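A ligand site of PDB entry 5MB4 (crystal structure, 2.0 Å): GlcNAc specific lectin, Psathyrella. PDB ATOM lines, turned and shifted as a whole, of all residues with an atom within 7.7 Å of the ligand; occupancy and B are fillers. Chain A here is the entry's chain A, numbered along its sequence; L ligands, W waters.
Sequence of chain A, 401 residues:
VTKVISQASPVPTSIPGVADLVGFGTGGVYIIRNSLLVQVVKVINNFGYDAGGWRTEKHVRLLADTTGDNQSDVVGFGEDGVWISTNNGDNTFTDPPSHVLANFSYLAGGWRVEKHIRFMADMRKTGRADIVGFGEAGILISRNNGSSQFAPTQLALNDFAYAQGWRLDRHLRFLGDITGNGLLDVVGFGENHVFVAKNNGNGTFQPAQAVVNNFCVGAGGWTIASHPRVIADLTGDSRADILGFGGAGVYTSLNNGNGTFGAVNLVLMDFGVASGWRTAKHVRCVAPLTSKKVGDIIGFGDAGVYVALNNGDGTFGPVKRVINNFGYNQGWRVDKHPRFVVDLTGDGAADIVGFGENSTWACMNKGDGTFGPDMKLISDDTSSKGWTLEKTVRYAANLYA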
ATOM      1  N   ASN A  45     -20.345  39.813 -19.323  1.00  0.00           N
ATOM      2  CA  ASN A  45     -20.527  39.926 -17.887  1.00  0.00           C
ATOM      3  C   ASN A  45     -21.487  38.847 -17.406  1.00  0.00           C
ATOM      4  O   ASN A  45     -22.520  39.137 -16.832  1.00  0.00           O
ATOM      5  CB  ASN A  45     -20.953  41.383 -17.542  1.00  0.00           C
ATOM      6  CG  ASN A  45     -20.982  41.667 -16.022  1.00  0.00           C
ATOM      7  OD1 ASN A  45     -21.858  42.420 -15.596  1.00  0.00           O
ATOM      8  ND2 ASN A  45     -20.059  41.107 -15.229  1.00  0.00           N
ATOM      9  N   ASN A  46     -21.128  37.586 -17.685  1.00  0.00           N
ATOM     10  CA  ASN A  46     -21.935  36.387 -17.396  1.00  0.00           C
ATOM     11  C   ASN A  46     -21.066  35.139 -17.519  1.00  0.00           C
ATOM     12  O   ASN A  46     -19.888  35.262 -17.801  1.00  0.00           O
ATOM     13  CB  ASN A  46     -23.146  36.257 -18.321  1.00  0.00           C
ATOM     14  CG  ASN A  46     -24.376  35.796 -17.570  1.00  0.00           C
ATOM     15  OD1 ASN A  46     -24.381  34.754 -16.928  1.00  0.00           O
ATOM     16  ND2 ASN A  46     -25.431  36.599 -17.665  1.00  0.00           N
ATOM     17  N   PHE A  47     -21.629  33.981 -17.265  1.00  0.00           N
ATOM     18  CA  PHE A  47     -20.870  32.721 -17.285  1.00  0.00           C
ATOM     19  C   PHE A  47     -19.730  32.626 -16.273  1.00  0.00           C
ATOM     20  O   PHE A  47     -18.825  31.785 -16.435  1.00  0.00           O
ATOM     21  CB  PHE A  47     -20.366  32.390 -18.689  1.00  0.00           C
ATOM     22  CG  PHE A  47     -21.457  32.329 -19.728  1.00  0.00           C
ATOM     23  CD1 PHE A  47     -22.282  31.212 -19.840  1.00  0.00           C
ATOM     24  CD2 PHE A  47     -21.692  33.393 -20.612  1.00  0.00           C
ATOM     25  CE1 PHE A  47     -23.261  31.158 -20.821  1.00  0.00           C
ATOM     26  CE2 PHE A  47     -22.680  33.342 -21.583  1.00  0.00           C
ATOM     27  CZ  PHE A  47     -23.467  32.210 -21.684  1.00  0.00           C
ATOM     28  N   GLY A  48     -19.828  33.433 -15.202  1.00  0.00           N
ATOM     29  CA  GLY A  48     -18.813  33.510 -14.177  1.00  0.00           C
ATOM     30  C   GLY A  48     -19.267  33.147 -12.769  1.00  0.00           C
ATOM     31  O   GLY A  48     -20.412  33.353 -12.422  1.00  0.00           O
ATOM     32  N   ALA A  51     -20.668  36.170 -11.648  1.00  0.00           N
ATOM     33  CA  ALA A  51     -21.364  36.847 -12.713  1.00  0.00           C
ATOM     34  C   ALA A  51     -22.320  35.804 -13.282  1.00  0.00           C
ATOM     35  O   ALA A  51     -22.047  35.147 -14.322  1.00  0.00           O
ATOM     36  CB  ALA A  51     -20.388  37.372 -13.763  1.00  0.00           C
ATOM     37  N   GLY A  52     -23.376  35.599 -12.490  1.00  0.00           N
ATOM     38  CA  GLY A  52     -24.448  34.718 -12.799  1.00  0.00           C
ATOM     39  C   GLY A  52     -24.439  33.468 -11.981  1.00  0.00           C
ATOM     40  O   GLY A  52     -25.290  32.607 -12.209  1.00  0.00           O
ATOM     41  N   GLY A  53     -23.524  33.348 -11.042  1.00  0.00           N
ATOM     42  CA  GLY A  53     -23.517  32.182 -10.127  1.00  0.00           C
ATOM     43  C   GLY A  53     -23.061  30.840 -10.742  1.00  0.00           C
ATOM     44  O   GLY A  53     -23.473  29.762 -10.293  1.00  0.00           O
ATOM     45  N   TRP A  54     -22.160  30.899 -11.719  1.00  0.00           N
ATOM     46  CA  TRP A  54     -21.729  29.701 -12.438  1.00  0.00           C
ATOM     47  C   TRP A  54     -20.767  28.923 -11.551  1.00  0.00           C
ATOM     48  O   TRP A  54     -19.939  29.521 -10.884  1.00  0.00           O
ATOM     49  CB  TRP A  54     -21.172  30.061 -13.860  1.00  0.00           C
ATOM     50  CG  TRP A  54     -22.253  30.526 -14.759  1.00  0.00           C
ATOM     51  CD1 TRP A  54     -22.925  31.733 -14.701  1.00  0.00           C
ATOM     52  CD2 TRP A  54     -22.899  29.771 -15.777  1.00  0.00           C
ATOM     53  NE1 TRP A  54     -23.893  31.787 -15.653  1.00  0.00           N
ATOM     54  CE2 TRP A  54     -23.916  30.582 -16.323  1.00  0.00           C
ATOM     55  CE3 TRP A  54     -22.694  28.503 -16.309  1.00  0.00           C
ATOM     56  CZ2 TRP A  54     -24.747  30.159 -17.341  1.00  0.00           C
ATOM     57  CZ3 TRP A  54     -23.532  28.083 -17.354  1.00  0.00           C
ATOM     58  CH2 TRP A  54     -24.545  28.919 -17.847  1.00  0.00           C
ATOM     59  N   ARG A  55     -20.915  27.593 -11.491  1.00  0.00           N
ATOM     60  CA  ARG A  55     -20.123  26.732 -10.645  1.00  0.00           C
ATOM     61  C   ARG A  55     -19.618  25.517 -11.401  1.00  0.00           C
ATOM     62  O   ARG A  55     -20.355  24.839 -12.145  1.00  0.00           O
ATOM     63  CB  ARG A  55     -20.920  26.220  -9.451  1.00  0.00           C
ATOM     64  CG  ARG A  55     -21.440  27.301  -8.541  1.00  0.00           C
ATOM     65  CD  ARG A  55     -20.365  27.819  -7.625  1.00  0.00           C
ATOM     66  NE  ARG A  55     -20.892  28.864  -6.739  1.00  0.00           N
ATOM     67  CZ  ARG A  55     -21.035  30.137  -7.047  1.00  0.00           C
ATOM     68  NH1 ARG A  55     -20.746  30.594  -8.233  1.00  0.00           N
ATOM     69  NH2 ARG A  55     -21.485  30.980  -6.127  1.00  0.00           N
ATOM     70  N   LYS A  58     -21.627  22.408 -10.760  1.00  0.00           N
ATOM     71  CA  LYS A  58     -23.006  22.258 -11.228  1.00  0.00           C
ATOM     72  C   LYS A  58     -23.275  22.594 -12.691  1.00  0.00           C
ATOM     73  O   LYS A  58     -24.379  22.256 -13.208  1.00  0.00           O
ATOM     74  CB  LYS A  58     -23.909  23.160 -10.369  1.00  0.00           C
ATOM     75  CG  LYS A  58     -23.917  22.858  -8.871  1.00  0.00           C
ATOM     76  CD  LYS A  58     -24.756  23.924  -8.162  1.00  0.00           C
ATOM     77  CE  LYS A  58     -26.239  23.563  -8.165  1.00  0.00           C
ATOM     78  NZ  LYS A  58     -27.210  24.638  -7.765  1.00  0.00           N
ATOM     79  N   HIS A  59     -22.367  23.313 -13.352  1.00  0.00           N
ATOM     80  CA  HIS A  59     -22.576  23.820 -14.677  1.00  0.00           C
ATOM     81  C   HIS A  59     -21.403  23.469 -15.603  1.00  0.00           C
ATOM     82  O   HIS A  59     -20.329  23.075 -15.130  1.00  0.00           O
ATOM     83  CB  HIS A  59     -22.800  25.329 -14.603  1.00  0.00           C
ATOM     84  CG  HIS A  59     -23.781  25.743 -13.547  1.00  0.00           C
ATOM     85  ND1 HIS A  59     -23.463  26.652 -12.565  1.00  0.00           N
ATOM     86  CD2 HIS A  59     -25.060  25.380 -13.289  1.00  0.00           C
ATOM     87  CE1 HIS A  59     -24.500  26.872 -11.783  1.00  0.00           C
ATOM     88  NE2 HIS A  59     -25.491  26.106 -12.200  1.00  0.00           N
ATOM     89  N   ARG A  61     -19.448  24.958 -19.189  1.00  0.00           N
ATOM     90  CA  ARG A  61     -19.194  26.085 -20.061  1.00  0.00           C
ATOM     91  C   ARG A  61     -18.234  25.665 -21.193  1.00  0.00           C
ATOM     92  O   ARG A  61     -17.148  25.095 -20.938  1.00  0.00           O
ATOM     93  CB  ARG A  61     -18.638  27.214 -19.212  1.00  0.00           C
ATOM     94  CG  ARG A  61     -19.729  27.866 -18.362  1.00  0.00           C
ATOM     95  CD  ARG A  61     -19.162  28.693 -17.205  1.00  0.00           C
ATOM     96  NE  ARG A  61     -18.601  27.844 -16.178  1.00  0.00           N
ATOM     97  CZ  ARG A  61     -18.032  28.321 -15.068  1.00  0.00           C
ATOM     98  NH1 ARG A  61     -17.928  29.629 -14.875  1.00  0.00           N
ATOM     99  NH2 ARG A  61     -17.536  27.491 -14.175  1.00  0.00           N
ATOM    100  N   GLY A  76     -23.371  27.878 -22.273  1.00  0.00           N
ATOM    101  CA  GLY A  76     -23.374  27.456 -20.854  1.00  0.00           C
ATOM    102  C   GLY A  76     -24.558  26.579 -20.529  1.00  0.00           C
ATOM    103  O   GLY A  76     -25.677  26.976 -20.798  1.00  0.00           O
ATOM    104  N   PHE A  77     -24.291  25.418 -19.935  1.00  0.00           N
ATOM    105  CA  PHE A  77     -25.358  24.574 -19.359  1.00  0.00           C
ATOM    106  C   PHE A  77     -25.520  24.996 -17.901  1.00  0.00           C
ATOM    107  O   PHE A  77     -24.751  24.597 -17.029  1.00  0.00           O
ATOM    108  CB  PHE A  77     -24.978  23.102 -19.435  1.00  0.00           C
ATOM    109  CG  PHE A  77     -24.776  22.604 -20.831  1.00  0.00           C
ATOM    110  CD1 PHE A  77     -23.591  22.835 -21.509  1.00  0.00           C
ATOM    111  CD2 PHE A  77     -25.793  21.968 -21.486  1.00  0.00           C
ATOM    112  CE1 PHE A  77     -23.403  22.387 -22.808  1.00  0.00           C
ATOM    113  CE2 PHE A  77     -25.610  21.528 -22.783  1.00  0.00           C
ATOM    114  CZ  PHE A  77     -24.397  21.725 -23.442  1.00  0.00           C
ATOM    115  N   GLY A  78     -26.523  25.839 -17.660  1.00  0.00           N
ATOM    116  CA  GLY A  78     -26.652  26.524 -16.385  1.00  0.00           C
ATOM    117  C   GLY A  78     -27.642  25.849 -15.440  1.00  0.00           C
ATOM    118  O   GLY A  78     -27.791  24.605 -15.432  1.00  0.00           O
ATOM    119  N   GLU A  79     -28.289  26.680 -14.621  1.00  0.00           N
ATOM    120  CA  GLU A  79     -29.170  26.149 -13.553  1.00  0.00           C
ATOM    121  C   GLU A  79     -30.521  25.628 -14.106  1.00  0.00           C
ATOM    122  O   GLU A  79     -31.002  24.558 -13.712  1.00  0.00           O
ATOM    123  CB  GLU A  79     -29.391  27.270 -12.500  1.00  0.00           C
ATOM    124  CG  GLU A  79     -29.928  26.833 -11.149  1.00  0.00           C
ATOM    125  CD  GLU A  79     -28.987  25.919 -10.349  1.00  0.00           C
ATOM    126  OE1 GLU A  79     -27.829  25.719 -10.735  1.00  0.00           O
ATOM    127  OE2 GLU A  79     -29.441  25.376  -9.318  1.00  0.00           O
ATOM    128  N   ASP A  80     -31.092  26.383 -15.030  1.00  0.00           N
ATOM    129  CA  ASP A  80     -32.433  26.174 -15.550  1.00  0.00           C
ATOM    130  C   ASP A  80     -32.535  25.948 -17.052  1.00  0.00           C
ATOM    131  O   ASP A  80     -33.660  25.785 -17.554  1.00  0.00           O
ATOM    132  CB  ASP A  80     -33.273  27.396 -15.165  1.00  0.00           C
ATOM    133  CG  ASP A  80     -33.395  27.530 -13.663  1.00  0.00           C
ATOM    134  OD1 ASP A  80     -33.776  26.537 -13.001  1.00  0.00           O
ATOM    135  OD2 ASP A  80     -33.029  28.599 -13.129  1.00  0.00           O
ATOM    136  N   GLY A  81     -31.399  25.900 -17.749  1.00  0.00           N
ATOM    137  CA  GLY A  81     -31.403  25.804 -19.192  1.00  0.00           C
ATOM    138  C   GLY A  81     -30.039  26.102 -19.832  1.00  0.00           C
ATOM    139  O   GLY A  81     -29.061  26.363 -19.134  1.00  0.00           O
ATOM    140  N   VAL A  82     -30.017  26.054 -21.160  1.00  0.00           N
ATOM    141  CA  VAL A  82     -28.792  26.262 -21.932  1.00  0.00           C
ATOM    142  C   VAL A  82     -28.796  27.708 -22.336  1.00  0.00           C
ATOM    143  O   VAL A  82     -29.787  28.188 -22.846  1.00  0.00           O
ATOM    144  CB  VAL A  82     -28.742  25.360 -23.168  1.00  0.00           C
ATOM    145  CG1 VAL A  82     -27.451  25.561 -23.937  1.00  0.00           C
ATOM    146  CG2 VAL A  82     -28.849  23.902 -22.749  1.00  0.00           C
ATOM    147  N   TRP A  83     -27.677  28.384 -22.095  1.00  0.00           N
ATOM    148  CA  TRP A  83     -27.521  29.813 -22.332  1.00  0.00           C
ATOM    149  C   TRP A  83     -26.436  30.041 -23.373  1.00  0.00           C
ATOM    150  O   TRP A  83     -25.347  29.461 -23.260  1.00  0.00           O
ATOM    151  CB  TRP A  83     -27.108  30.510 -21.049  1.00  0.00           C
ATOM    152  CG  TRP A  83     -28.206  30.603 -20.020  1.00  0.00           C
ATOM    153  CD1 TRP A  83     -28.507  29.695 -19.034  1.00  0.00           C
ATOM    154  CD2 TRP A  83     -29.114  31.681 -19.850  1.00  0.00           C
ATOM    155  NE1 TRP A  83     -29.551  30.147 -18.273  1.00  0.00           N
ATOM    156  CE2 TRP A  83     -29.958  31.353 -18.773  1.00  0.00           C
ATOM    157  CE3 TRP A  83     -29.303  32.898 -20.512  1.00  0.00           C
ATOM    158  CZ2 TRP A  83     -30.954  32.204 -18.313  1.00  0.00           C
ATOM    159  CZ3 TRP A  83     -30.332  33.761 -20.086  1.00  0.00           C
ATOM    160  CH2 TRP A  83     -31.125  33.407 -18.974  1.00  0.00           C
ATOM    161  N   PRO A  96     -26.665  40.483 -22.516  1.00  0.00           N
ATOM    162  CA  PRO A  96     -26.626  39.176 -21.865  1.00  0.00           C
ATOM    163  C   PRO A  96     -26.855  37.998 -22.807  1.00  0.00           C
ATOM    164  O   PRO A  96     -27.396  38.211 -23.898  1.00  0.00           O
ATOM    165  CB  PRO A  96     -27.789  39.270 -20.854  1.00  0.00           C
ATOM    166  CG  PRO A  96     -28.793  40.135 -21.576  1.00  0.00           C
ATOM    167  CD  PRO A  96     -27.951  41.171 -22.264  1.00  0.00           C
ATOM    168  N   PRO A  97     -26.451  36.773 -22.382  1.00  0.00           N
ATOM    169  CA  PRO A  97     -26.759  35.683 -23.250  1.00  0.00           C
ATOM    170  C   PRO A  97     -28.256  35.407 -23.286  1.00  0.00           C
ATOM    171  O   PRO A  97     -29.029  35.940 -22.511  1.00  0.00           O
ATOM    172  CB  PRO A  97     -26.030  34.502 -22.629  1.00  0.00           C
ATOM    173  CG  PRO A  97     -25.985  34.805 -21.187  1.00  0.00           C
ATOM    174  CD  PRO A  97     -25.854  36.306 -21.108  1.00  0.00           C
ATOM    175  N   HIS A  99     -31.310  32.373 -23.359  1.00  0.00           N
ATOM    176  CA  HIS A  99     -31.626  31.009 -22.926  1.00  0.00           C
ATOM    177  C   HIS A  99     -32.375  30.317 -24.057  1.00  0.00           C
ATOM    178  O   HIS A  99     -33.475  30.675 -24.364  1.00  0.00           O
ATOM    179  CB  HIS A  99     -32.417  31.129 -21.632  1.00  0.00           C
ATOM    180  CG  HIS A  99     -32.887  29.840 -21.068  1.00  0.00           C
ATOM    181  ND1 HIS A  99     -33.349  29.732 -19.782  1.00  0.00           N
ATOM    182  CD2 HIS A  99     -33.049  28.630 -21.635  1.00  0.00           C
ATOM    183  CE1 HIS A  99     -33.779  28.503 -19.577  1.00  0.00           C
ATOM    184  NE2 HIS A  99     -33.592  27.822 -20.684  1.00  0.00           N
ATOM    185  N   SER A 105     -29.807  20.846 -17.908  1.00  0.00           N
ATOM    186  CA  SER A 105     -29.410  21.738 -16.809  1.00  0.00           C
ATOM    187  C   SER A 105     -29.737  21.131 -15.465  1.00  0.00           C
ATOM    188  O   SER A 105     -30.423  20.092 -15.402  1.00  0.00           O
ATOM    189  CB  SER A 105     -30.056  23.104 -16.972  1.00  0.00           C
ATOM    190  OG  SER A 105     -31.419  23.019 -16.585  1.00  0.00           O
HETATM  191  C1  LIG L   1     -29.025  32.463 -13.858  1.00  0.00           C
HETATM  192  C2  LIG L   1     -27.881  32.166 -14.830  1.00  0.00           C
HETATM  193  C3  LIG L   1     -27.316  33.455 -15.397  1.00  0.00           C
HETATM  194  C4  LIG L   1     -28.424  34.345 -15.955  1.00  0.00           C
HETATM  195  C5  LIG L   1     -29.569  34.463 -14.947  1.00  0.00           C
HETATM  196  C6  LIG L   1     -30.762  35.218 -15.561  1.00  0.00           C
HETATM  197  C7  LIG L   1     -26.821  30.092 -14.256  1.00  0.00           C
HETATM  198  C8  LIG L   1     -25.687  29.442 -13.536  1.00  0.00           C
HETATM  199  N1  LIG L   1     -26.849  31.413 -14.194  1.00  0.00           N
HETATM  200  O1  LIG L   1     -29.655  31.263 -13.559  1.00  0.00           O
HETATM  201  O2  LIG L   1     -26.411  33.183 -16.435  1.00  0.00           O
HETATM  202  O3  LIG L   1     -27.894  35.629 -16.168  1.00  0.00           O
HETATM  203  O4  LIG L   1     -30.024  33.197 -14.526  1.00  0.00           O
HETATM  204  O5  LIG L   1     -31.741  35.432 -14.567  1.00  0.00           O
HETATM  205  O6  LIG L   1     -27.653  29.398 -14.842  1.00  0.00           O
HETATM  206  O   HOH W   1     -32.247  30.762 -14.941  1.00  0.00           O
HETATM  207  O   HOH W   2     -30.260  29.194 -15.826  1.00  0.00           O
HETATM  208  O   HOH W   3     -26.762  37.210 -14.096  1.00  0.00           O
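An oxygen (O2) of the ligand lies within hydrogen-bond range of the side-chain amide oxygen of Asn 46 (2.6 Å).
O of Gly 52 lies within hydrogen-bond range of N1 of the ligand (2.8 Å).
The backbone NH of Glu 79 sits at hydrogen-bond distance from an oxygen (O6) of the ligand.
The indole nitrogen (NE1) of Trp 54 is in hydrogen-bond range of an oxygen (O2) of the ligand.
NE1 of Trp 54 lies within hydrogen-bond range of OD1 of Asn 46, at 3.3 Å.
OE1 of Glu 79 is in hydrogen-bond range of NE2 of His 59.
O of Glu 79 sits at hydrogen-bond distance from OG of Ser 105 (3.3 Å).
The side-chain carboxylate (OE2) of Glu 79 is in salt-bridge range of the side-chain amino group (NZ) of Lys 58 (2.8 Å).
N of Trp 54 is in hydrogen-bond range of O of Gly 48.
The backbone NH (N) of Arg 55 lies within hydrogen-bond range of a ring nitrogen (ND1) of His 59 (2.9 Å).
O of Trp 83 sits at hydrogen-bond distance from N of Gly 76 (2.7 Å).
The backbone NH of Gly 53 sits at hydrogen-bond distance from the backbone carbonyl oxygen of Gly 48, at 3.4 Å.
Merely in contact with the ligand: Gly 53 (3.9 Å), His 59 (3.3 Å), Gly 78 (3.4 Å) and Trp 83 (3.9 Å).
Hydrophobic or aromatic side chains that line the ligand: Trp 54, His 59 and Trp 83.
Within 4 Å of the ligand: Asn 46, Gly 52, Gly 53, Trp 54, His 59, Gly 78, Glu 79 and Trp 83.
The nearest printed residue that does not touch the ligand is Asp 80 (4.3 Å).
Water W1 bridges OD2 of Asp 80 (2.9 Å) and O1 of the ligand (3.0 Å).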
